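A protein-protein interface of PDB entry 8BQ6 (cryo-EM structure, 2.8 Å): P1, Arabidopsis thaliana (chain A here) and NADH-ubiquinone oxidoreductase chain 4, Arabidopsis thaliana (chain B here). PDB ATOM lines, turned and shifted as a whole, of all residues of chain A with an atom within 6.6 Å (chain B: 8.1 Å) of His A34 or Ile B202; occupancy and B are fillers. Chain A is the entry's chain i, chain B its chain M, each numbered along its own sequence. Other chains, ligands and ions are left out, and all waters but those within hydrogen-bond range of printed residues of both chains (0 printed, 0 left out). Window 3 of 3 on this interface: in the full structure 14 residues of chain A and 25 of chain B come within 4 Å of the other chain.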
ATOM      1  N   HIS A  29       7.918  -9.309  -9.135  1.00  0.00           N
ATOM      2  CA  HIS A  29       8.718  -9.081  -7.938  1.00  0.00           C
ATOM      3  C   HIS A  29      10.039  -9.842  -8.023  1.00  0.00           C
ATOM      4  O   HIS A  29      11.123  -9.263  -7.847  1.00  0.00           O
ATOM      5  CB  HIS A  29       7.904  -9.480  -6.704  1.00  0.00           C
ATOM      6  CG  HIS A  29       8.707  -9.598  -5.449  1.00  0.00           C
ATOM      7  ND1 HIS A  29       8.919  -8.534  -4.599  1.00  0.00           N
ATOM      8  CD2 HIS A  29       9.320 -10.663  -4.879  1.00  0.00           C
ATOM      9  CE1 HIS A  29       9.647  -8.933  -3.572  1.00  0.00           C
ATOM     10  NE2 HIS A  29       9.901 -10.221  -3.716  1.00  0.00           N
ATOM     11  N   ILE A  30       9.966 -11.127  -8.378  1.00  0.00           N
ATOM     12  CA  ILE A  30      11.162 -11.959  -8.481  1.00  0.00           C
ATOM     13  C   ILE A  30      12.070 -11.472  -9.606  1.00  0.00           C
ATOM     14  O   ILE A  30      13.291 -11.350  -9.432  1.00  0.00           O
ATOM     15  CB  ILE A  30      10.763 -13.430  -8.680  1.00  0.00           C
ATOM     16  CG1 ILE A  30       9.745 -13.846  -7.618  1.00  0.00           C
ATOM     17  CG2 ILE A  30      11.985 -14.320  -8.636  1.00  0.00           C
ATOM     18  CD1 ILE A  30       9.745 -15.324  -7.313  1.00  0.00           C
ATOM     19  N   TYR A  31      11.492 -11.206 -10.786  1.00  0.00           N
ATOM     20  CA  TYR A  31      12.311 -10.787 -11.924  1.00  0.00           C
ATOM     21  C   TYR A  31      13.100  -9.522 -11.607  1.00  0.00           C
ATOM     22  O   TYR A  31      14.335  -9.483 -11.766  1.00  0.00           O
ATOM     23  CB  TYR A  31      11.425 -10.573 -13.154  1.00  0.00           C
ATOM     24  CG  TYR A  31      12.171 -10.163 -14.410  1.00  0.00           C
ATOM     25  CD1 TYR A  31      13.107 -11.005 -15.000  1.00  0.00           C
ATOM     26  CD2 TYR A  31      11.928  -8.934 -15.012  1.00  0.00           C
ATOM     27  CE1 TYR A  31      13.785 -10.626 -16.154  1.00  0.00           C
ATOM     28  CE2 TYR A  31      12.596  -8.551 -16.159  1.00  0.00           C
ATOM     29  CZ  TYR A  31      13.523  -9.396 -16.726  1.00  0.00           C
ATOM     30  OH  TYR A  31      14.185  -8.997 -17.866  1.00  0.00           O
ATOM     31  N   GLU A  32      12.408  -8.483 -11.137  1.00  0.00           N
ATOM     32  CA  GLU A  32      13.085  -7.233 -10.839  1.00  0.00           C
ATOM     33  C   GLU A  32      14.089  -7.365  -9.705  1.00  0.00           C
ATOM     34  O   GLU A  32      15.185  -6.814  -9.824  1.00  0.00           O
ATOM     35  CB  GLU A  32      12.080  -6.117 -10.532  1.00  0.00           C
ATOM     36  CG  GLU A  32      10.824  -6.120 -11.397  1.00  0.00           C
ATOM     37  CD  GLU A  32      11.047  -5.567 -12.798  1.00  0.00           C
ATOM     38  OE1 GLU A  32      10.046  -5.248 -13.475  1.00  0.00           O
ATOM     39  OE2 GLU A  32      12.213  -5.460 -13.232  1.00  0.00           O
ATOM     40  N   MET A  33      13.782  -8.091  -8.629  1.00  0.00           N
ATOM     41  CA  MET A  33      14.778  -8.211  -7.567  1.00  0.00           C
ATOM     42  C   MET A  33      16.009  -8.982  -7.988  1.00  0.00           C
ATOM     43  O   MET A  33      17.116  -8.638  -7.560  1.00  0.00           O
ATOM     44  CB  MET A  33      14.154  -8.838  -6.320  1.00  0.00           C
ATOM     45  CG  MET A  33      13.085  -7.978  -5.648  1.00  0.00           C
ATOM     46  SD  MET A  33      13.650  -6.362  -5.077  1.00  0.00           S
ATOM     47  CE  MET A  33      14.785  -6.796  -3.753  1.00  0.00           C
ATOM     48  N   HIS A  34      15.852  -9.986  -8.847  1.00  0.00           N
ATOM     49  CA  HIS A  34      17.014 -10.751  -9.270  1.00  0.00           C
ATOM     50  C   HIS A  34      17.897  -9.952 -10.219  1.00  0.00           C
ATOM     51  O   HIS A  34      19.126 -10.096 -10.197  1.00  0.00           O
ATOM     52  CB  HIS A  34      16.564 -12.062  -9.899  1.00  0.00           C
ATOM     53  CG  HIS A  34      16.290 -13.129  -8.890  1.00  0.00           C
ATOM     54  ND1 HIS A  34      17.032 -13.264  -7.736  1.00  0.00           N
ATOM     55  CD2 HIS A  34      15.337 -14.086  -8.839  1.00  0.00           C
ATOM     56  CE1 HIS A  34      16.565 -14.277  -7.031  1.00  0.00           C
ATOM     57  NE2 HIS A  34      15.533 -14.791  -7.675  1.00  0.00           N
ATOM     58  N   GLU A  35      17.308  -9.095 -11.054  1.00  0.00           N
ATOM     59  CA  GLU A  35      18.198  -8.228 -11.823  1.00  0.00           C
ATOM     60  C   GLU A  35      18.630  -6.984 -11.057  1.00  0.00           C
ATOM     61  O   GLU A  35      19.519  -6.263 -11.524  1.00  0.00           O
ATOM     62  CB  GLU A  35      17.567  -7.822 -13.153  1.00  0.00           C
ATOM     63  CG  GLU A  35      16.247  -7.106 -13.060  1.00  0.00           C
ATOM     64  CD  GLU A  35      15.369  -7.467 -14.226  1.00  0.00           C
ATOM     65  OE1 GLU A  35      15.516  -8.604 -14.717  1.00  0.00           O
ATOM     66  OE2 GLU A  35      14.555  -6.628 -14.661  1.00  0.00           O
ATOM     67  N   ARG A  36      18.044  -6.730  -9.890  1.00  0.00           N
ATOM     68  CA  ARG A  36      18.356  -5.557  -9.090  1.00  0.00           C
ATOM     69  C   ARG A  36      19.386  -5.836  -8.001  1.00  0.00           C
ATOM     70  O   ARG A  36      20.016  -4.896  -7.507  1.00  0.00           O
ATOM     71  CB  ARG A  36      17.049  -5.026  -8.478  1.00  0.00           C
ATOM     72  CG  ARG A  36      17.139  -3.725  -7.695  1.00  0.00           C
ATOM     73  CD  ARG A  36      15.805  -3.312  -7.091  1.00  0.00           C
ATOM     74  NE  ARG A  36      14.809  -2.996  -8.110  1.00  0.00           N
ATOM     75  CZ  ARG A  36      14.696  -1.820  -8.713  1.00  0.00           C
ATOM     76  NH1 ARG A  36      15.485  -0.804  -8.406  1.00  0.00           N
ATOM     77  NH2 ARG A  36      13.761  -1.657  -9.645  1.00  0.00           N
ATOM     78  N   CYS A  37      19.598  -7.102  -7.646  1.00  0.00           N
ATOM     79  CA  CYS A  37      20.454  -7.507  -6.521  1.00  0.00           C
ATOM     80  C   CYS A  37      21.925  -7.090  -6.669  1.00  0.00           C
ATOM     81  O   CYS A  37      22.722  -7.403  -5.768  1.00  0.00           O
ATOM     82  CB  CYS A  37      20.364  -9.022  -6.330  1.00  0.00           C
ATOM     83  SG  CYS A  37      21.292 -10.010  -7.531  1.00  0.00           S
ATOM     84  N   LYS A  38      22.306  -6.409  -7.748  1.00  0.00           N
ATOM     85  CA  LYS A  38      23.696  -6.061  -7.996  1.00  0.00           C
ATOM     86  C   LYS A  38      24.059  -4.635  -7.603  1.00  0.00           C
ATOM     87  O   LYS A  38      25.226  -4.382  -7.285  1.00  0.00           O
ATOM     88  CB  LYS A  38      24.023  -6.258  -9.481  1.00  0.00           C
ATOM     89  CG  LYS A  38      23.899  -7.700  -9.944  1.00  0.00           C
ATOM     90  CD  LYS A  38      24.669  -8.640  -9.030  1.00  0.00           C
ATOM     91  CE  LYS A  38      26.172  -8.392  -9.089  1.00  0.00           C
ATOM     92  NZ  LYS A  38      26.634  -7.826 -10.388  1.00  0.00           N
ATOM     93  N   PHE B  66       2.024 -16.548  -2.282  1.00  0.00           N
ATOM     94  CA  PHE B  66       1.602 -15.838  -1.087  1.00  0.00           C
ATOM     95  C   PHE B  66       0.385 -14.990  -1.435  1.00  0.00           C
ATOM     96  O   PHE B  66       0.352 -14.349  -2.490  1.00  0.00           O
ATOM     97  CB  PHE B  66       2.749 -14.980  -0.559  1.00  0.00           C
ATOM     98  CG  PHE B  66       3.870 -15.774   0.048  1.00  0.00           C
ATOM     99  CD1 PHE B  66       3.666 -16.549   1.176  1.00  0.00           C
ATOM    100  CD2 PHE B  66       5.115 -15.799  -0.555  1.00  0.00           C
ATOM    101  CE1 PHE B  66       4.706 -17.281   1.719  1.00  0.00           C
ATOM    102  CE2 PHE B  66       6.150 -16.542  -0.022  1.00  0.00           C
ATOM    103  CZ  PHE B  66       5.944 -17.285   1.116  1.00  0.00           C
ATOM    104  N   TYR B  83       7.402  -6.894   2.701  1.00  0.00           N
ATOM    105  CA  TYR B  83       6.170  -7.474   2.192  1.00  0.00           C
ATOM    106  C   TYR B  83       5.475  -8.272   3.285  1.00  0.00           C
ATOM    107  O   TYR B  83       6.129  -8.882   4.137  1.00  0.00           O
ATOM    108  CB  TYR B  83       6.447  -8.378   0.984  1.00  0.00           C
ATOM    109  CG  TYR B  83       7.063  -7.655  -0.189  1.00  0.00           C
ATOM    110  CD1 TYR B  83       8.391  -7.248  -0.158  1.00  0.00           C
ATOM    111  CD2 TYR B  83       6.319  -7.371  -1.324  1.00  0.00           C
ATOM    112  CE1 TYR B  83       8.957  -6.583  -1.217  1.00  0.00           C
ATOM    113  CE2 TYR B  83       6.879  -6.704  -2.393  1.00  0.00           C
ATOM    114  CZ  TYR B  83       8.199  -6.313  -2.333  1.00  0.00           C
ATOM    115  OH  TYR B  83       8.770  -5.651  -3.394  1.00  0.00           O
ATOM    116  N   LEU B 137       6.936 -11.577   5.400  1.00  0.00           N
ATOM    117  CA  LEU B 137       7.649 -12.211   4.298  1.00  0.00           C
ATOM    118  C   LEU B 137       9.104 -11.774   4.232  1.00  0.00           C
ATOM    119  O   LEU B 137       9.672 -11.647   3.141  1.00  0.00           O
ATOM    120  CB  LEU B 137       6.948 -11.941   2.969  1.00  0.00           C
ATOM    121  CG  LEU B 137       5.537 -12.513   2.855  1.00  0.00           C
ATOM    122  CD1 LEU B 137       5.138 -12.610   1.399  1.00  0.00           C
ATOM    123  CD2 LEU B 137       5.466 -13.873   3.521  1.00  0.00           C
ATOM    124  N   THR B 195      23.271 -12.647  -0.302  1.00  0.00           N
ATOM    125  CA  THR B 195      22.209 -12.350  -1.247  1.00  0.00           C
ATOM    126  C   THR B 195      21.976 -10.861  -1.434  1.00  0.00           C
ATOM    127  O   THR B 195      21.413 -10.463  -2.458  1.00  0.00           O
ATOM    128  CB  THR B 195      20.918 -13.027  -0.791  1.00  0.00           C
ATOM    129  OG1 THR B 195      20.401 -12.347   0.357  1.00  0.00           O
ATOM    130  CG2 THR B 195      21.189 -14.479  -0.428  1.00  0.00           C
ATOM    131  N   GLY B 196      22.391 -10.033  -0.481  1.00  0.00           N
ATOM    132  CA  GLY B 196      22.072  -8.627  -0.550  1.00  0.00           C
ATOM    133  C   GLY B 196      20.624  -8.306  -0.271  1.00  0.00           C
ATOM    134  O   GLY B 196      20.198  -7.174  -0.518  1.00  0.00           O
ATOM    135  N   THR B 197      19.854  -9.265   0.234  1.00  0.00           N
ATOM    136  CA  THR B 197      18.440  -9.058   0.491  1.00  0.00           C
ATOM    137  C   THR B 197      18.006  -9.957   1.639  1.00  0.00           C
ATOM    138  O   THR B 197      18.709 -10.895   2.025  1.00  0.00           O
ATOM    139  CB  THR B 197      17.591  -9.337  -0.756  1.00  0.00           C
ATOM    140  OG1 THR B 197      16.279  -8.788  -0.581  1.00  0.00           O
ATOM    141  CG2 THR B 197      17.480 -10.829  -1.003  1.00  0.00           C
ATOM    142  N   THR B 198      16.844  -9.632   2.199  1.00  0.00           N
ATOM    143  CA  THR B 198      16.188 -10.465   3.197  1.00  0.00           C
ATOM    144  C   THR B 198      14.766 -10.816   2.790  1.00  0.00           C
ATOM    145  O   THR B 198      14.001 -11.318   3.619  1.00  0.00           O
ATOM    146  CB  THR B 198      16.175  -9.772   4.563  1.00  0.00           C
ATOM    147  OG1 THR B 198      15.546  -8.489   4.445  1.00  0.00           O
ATOM    148  CG2 THR B 198      17.581  -9.605   5.100  1.00  0.00           C
ATOM    149  N   ASP B 199      14.391 -10.562   1.542  1.00  0.00           N
ATOM    150  CA  ASP B 199      13.040 -10.861   1.098  1.00  0.00           C
ATOM    151  C   ASP B 199      12.871 -12.367   0.958  1.00  0.00           C
ATOM    152  O   ASP B 199      13.620 -13.014   0.225  1.00  0.00           O
ATOM    153  CB  ASP B 199      12.748 -10.158  -0.221  1.00  0.00           C
ATOM    154  CG  ASP B 199      11.375 -10.480  -0.750  1.00  0.00           C
ATOM    155  OD1 ASP B 199      11.222 -11.511  -1.436  1.00  0.00           O
ATOM    156  OD2 ASP B 199      10.439  -9.713  -0.454  1.00  0.00           O
ATOM    157  N   LEU B 200      11.864 -12.914   1.634  1.00  0.00           N
ATOM    158  CA  LEU B 200      11.713 -14.364   1.715  1.00  0.00           C
ATOM    159  C   LEU B 200      11.518 -14.985   0.338  1.00  0.00           C
ATOM    160  O   LEU B 200      12.129 -16.014   0.020  1.00  0.00           O
ATOM    161  CB  LEU B 200      10.538 -14.694   2.630  1.00  0.00           C
ATOM    162  CG  LEU B 200      10.033 -16.126   2.736  1.00  0.00           C
ATOM    163  CD1 LEU B 200      11.073 -17.001   3.394  1.00  0.00           C
ATOM    164  CD2 LEU B 200       8.748 -16.117   3.528  1.00  0.00           C
ATOM    165  N   GLN B 201      10.686 -14.361  -0.499  1.00  0.00           N
ATOM    166  CA  GLN B 201      10.393 -14.910  -1.818  1.00  0.00           C
ATOM    167  C   GLN B 201      11.648 -15.018  -2.672  1.00  0.00           C
ATOM    168  O   GLN B 201      11.801 -15.972  -3.444  1.00  0.00           O
ATOM    169  CB  GLN B 201       9.351 -14.042  -2.516  1.00  0.00           C
ATOM    170  CG  GLN B 201       8.046 -13.941  -1.772  1.00  0.00           C
ATOM    171  CD  GLN B 201       6.953 -13.348  -2.623  1.00  0.00           C
ATOM    172  OE1 GLN B 201       6.532 -13.941  -3.616  1.00  0.00           O
ATOM    173  NE2 GLN B 201       6.498 -12.156  -2.254  1.00  0.00           N
ATOM    174  N   ILE B 202      12.548 -14.039  -2.570  1.00  0.00           N
ATOM    175  CA  ILE B 202      13.810 -14.125  -3.299  1.00  0.00           C
ATOM    176  C   ILE B 202      14.671 -15.253  -2.742  1.00  0.00           C
ATOM    177  O   ILE B 202      15.274 -16.022  -3.499  1.00  0.00           O
ATOM    178  CB  ILE B 202      14.549 -12.776  -3.267  1.00  0.00           C
ATOM    179  CG1 ILE B 202      13.662 -11.664  -3.832  1.00  0.00           C
ATOM    180  CG2 ILE B 202      15.842 -12.866  -4.047  1.00  0.00           C
ATOM    181  CD1 ILE B 202      13.058 -11.987  -5.178  1.00  0.00           C
ATOM    182  N   LEU B 203      14.732 -15.376  -1.411  1.00  0.00           N
ATOM    183  CA  LEU B 203      15.543 -16.428  -0.803  1.00  0.00           C
ATOM    184  C   LEU B 203      15.089 -17.818  -1.229  1.00  0.00           C
ATOM    185  O   LEU B 203      15.925 -18.703  -1.441  1.00  0.00           O
ATOM    186  CB  LEU B 203      15.513 -16.329   0.722  1.00  0.00           C
ATOM    187  CG  LEU B 203      16.437 -15.335   1.429  1.00  0.00           C
ATOM    188  CD1 LEU B 203      17.855 -15.465   0.911  1.00  0.00           C
ATOM    189  CD2 LEU B 203      15.977 -13.923   1.319  1.00  0.00           C
ATOM    190  N   LEU B 204      13.778 -18.004  -1.389  1.00  0.00           N
ATOM    191  CA  LEU B 204      13.230 -19.316  -1.825  1.00  0.00           C
ATOM    192  C   LEU B 204      13.662 -19.640  -3.262  1.00  0.00           C
ATOM    193  O   LEU B 204      13.486 -20.788  -3.687  1.00  0.00           O
ATOM    194  CB  LEU B 204      11.707 -19.237  -1.704  1.00  0.00           C
ATOM    195  CG  LEU B 204      11.184 -19.094  -0.275  1.00  0.00           C
ATOM    196  CD1 LEU B 204       9.666 -19.042  -0.245  1.00  0.00           C
ATOM    197  CD2 LEU B 204      11.708 -20.207   0.618  1.00  0.00           C
ATOM    198  N   THR B 205      14.192 -18.666  -3.997  1.00  0.00           N
ATOM    199  CA  THR B 205      14.635 -18.866  -5.370  1.00  0.00           C
ATOM    200  C   THR B 205      16.150 -18.778  -5.528  1.00  0.00           C
ATOM    201  O   THR B 205      16.640 -18.755  -6.663  1.00  0.00           O
ATOM    202  CB  THR B 205      13.961 -17.844  -6.283  1.00  0.00           C
ATOM    203  OG1 THR B 205      14.473 -16.542  -5.979  1.00  0.00           O
ATOM    204  CG2 THR B 205      12.461 -17.852  -6.075  1.00  0.00           C
ATOM    205  N   THR B 206      16.901 -18.733  -4.434  1.00  0.00           N
ATOM    206  CA  THR B 206      18.351 -18.633  -4.491  1.00  0.00           C
ATOM    207  C   THR B 206      18.986 -19.936  -4.020  1.00  0.00           C
ATOM    208  O   THR B 206      18.464 -20.631  -3.144  1.00  0.00           O
ATOM    209  CB  THR B 206      18.851 -17.460  -3.641  1.00  0.00           C
ATOM    210  OG1 THR B 206      18.024 -16.316  -3.879  1.00  0.00           O
ATOM    211  CG2 THR B 206      20.276 -17.099  -4.016  1.00  0.00           C
ATOM    212  N   GLU B 207      20.125 -20.266  -4.623  1.00  0.00           N
ATOM    213  CA  GLU B 207      20.833 -21.511  -4.356  1.00  0.00           C
ATOM    214  C   GLU B 207      21.910 -21.264  -3.307  1.00  0.00           C
ATOM    215  O   GLU B 207      22.633 -20.263  -3.371  1.00  0.00           O
ATOM    216  CB  GLU B 207      21.432 -22.080  -5.646  1.00  0.00           C
ATOM    217  CG  GLU B 207      22.487 -21.215  -6.319  1.00  0.00           C
ATOM    218  CD  GLU B 207      22.941 -21.788  -7.646  1.00  0.00           C
ATOM    219  OE1 GLU B 207      22.707 -22.992  -7.884  1.00  0.00           O
ATOM    220  OE2 GLU B 207      23.540 -21.037  -8.442  1.00  0.00           O
ATOM    221  N   PHE B 208      21.989 -22.159  -2.327  1.00  0.00           N
ATOM    222  CA  PHE B 208      23.009 -22.124  -1.288  1.00  0.00           C
ATOM    223  C   PHE B 208      23.944 -23.315  -1.450  1.00  0.00           C
ATOM    224  O   PHE B 208      23.549 -24.361  -1.972  1.00  0.00           O
ATOM    225  CB  PHE B 208      22.375 -22.149   0.106  1.00  0.00           C
ATOM    226  CG  PHE B 208      21.687 -20.870   0.498  1.00  0.00           C
ATOM    227  CD1 PHE B 208      22.422 -19.777   0.928  1.00  0.00           C
ATOM    228  CD2 PHE B 208      20.307 -20.759   0.436  1.00  0.00           C
ATOM    229  CE1 PHE B 208      21.796 -18.600   1.296  1.00  0.00           C
ATOM    230  CE2 PHE B 208      19.674 -19.581   0.796  1.00  0.00           C
ATOM    231  CZ  PHE B 208      20.420 -18.501   1.228  1.00  0.00           C
ATOM    232  N   MET B 271      14.352 -23.275   2.713  1.00  0.00           N
ATOM    233  CA  MET B 271      15.499 -22.467   2.214  1.00  0.00           C
ATOM    234  C   MET B 271      16.771 -23.317   2.121  1.00  0.00           C
ATOM    235  O   MET B 271      17.603 -23.007   1.247  1.00  0.00           O
ATOM    236  CB  MET B 271      15.781 -21.262   3.111  1.00  0.00           C
ATOM    237  CG  MET B 271      15.300 -19.952   2.520  1.00  0.00           C
ATOM    238  SD  MET B 271      15.052 -18.676   3.776  1.00  0.00           S
ATOM    239  CE  MET B 271      16.607 -18.778   4.656  1.00  0.00           C
ATOM    240  N   HIS B 491       9.851 -28.254  -2.459  1.00  0.00           N
ATOM    241  CA  HIS B 491      10.842 -27.157  -2.594  1.00  0.00           C
ATOM    242  C   HIS B 491      12.268 -27.694  -2.607  1.00  0.00           C
ATOM    243  O   HIS B 491      12.684 -28.305  -1.604  1.00  0.00           O
ATOM    244  CB  HIS B 491      10.624 -26.120  -1.493  1.00  0.00           C
ATOM    245  CG  HIS B 491      11.200 -24.794  -1.835  1.00  0.00           C
ATOM    246  ND1 HIS B 491      10.438 -23.786  -2.377  1.00  0.00           N
ATOM    247  CD2 HIS B 491      12.459 -24.323  -1.747  1.00  0.00           C
ATOM    248  CE1 HIS B 491      11.203 -22.740  -2.597  1.00  0.00           C
ATOM    249  NE2 HIS B 491      12.445 -23.043  -2.210  1.00  0.00           N
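Of the 10 printed residues of chain A, 4 touch a printed residue of chain B.
Hydrophobic or aromatic side chains of chain A that line the printed part of chain B: His A29, Ile A30, Met A33 and His A34.
Of the 19 printed residues of chain B, 4 touch a printed residue of chain A.
Among the printed residues, no Asp or Glu carboxylate lies within 4 Å of a Lys or Arg side-chain nitrogen of the other chain.
His A29 touches Ile B202.
Ile B202 touches Ile A30 (CD1 to CA, 3.8 Å).
Ile A30 touches Thr B205 (CD1 to CG2, 3.9 Å).
Ile B202 touches Met A33.
CE1 of His A34 touches CG2 of Ile B202, 3.4 Å away.
A ring nitrogen (NE2) of His A29 lies within hydrogen-bond range of the side-chain carboxylate (OD1) of Asp B199 (2.9 Å).
A ring nitrogen (NE2) of His A34 lies within hydrogen-bond range of the side-chain hydroxyl (OG1) of Thr B205 (2.7 Å).
OH of Tyr B83 lies within hydrogen-bond range of ND1 of His A29 (3.1 Å).
The side-chain hydroxyl (OG1) of Thr B197 sits at hydrogen-bond distance from the backbone NH (N) of Asp B199 (3.3 Å).
The backbone NH (N) of Leu B137 sits at hydrogen-bond distance from the backbone carbonyl oxygen (O) of Tyr B83 (3.1 Å).
N of Ile B202 sits at hydrogen-bond distance from OD1 of Asp B199.
SG of Cys A37 lies within hydrogen-bond range of O of His A34, 3.4 Å away.
The backbone carbonyl oxygen (O) of Ile B202 is in hydrogen-bond range of the side-chain hydroxyl (OG1) of Thr B205 (2.7 Å).
The side-chain hydroxyl (OG1) of Thr B206 is in hydrogen-bond range of the backbone carbonyl oxygen (O) of Ile B202 (2.8 Å).
Of the printed residues of chain B, His A34 touches Ile B202 and Thr B205.
Of chain A, only His A29, Ile A30, Met A33 and His A34 come within 4 Å of Ile B202.
Of the printed residues of chain A, Tyr B83 touches His A29.
Of the printed residues of chain B, Met A33 touches Ile B202 (3.5 Å).
Of the printed residues of chain A, Asp B199 touches His A29.
Gly B196 touches none of the printed residues of chain A.
Phe B208 touches none of the printed residues of chain A.
The nearest residue of chain B that does not touch His A34 is Thr B206 (4.03 Å).
The nearest residue of chain A that does not touch Ile B202 is Tyr A31 (5.9 Å).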
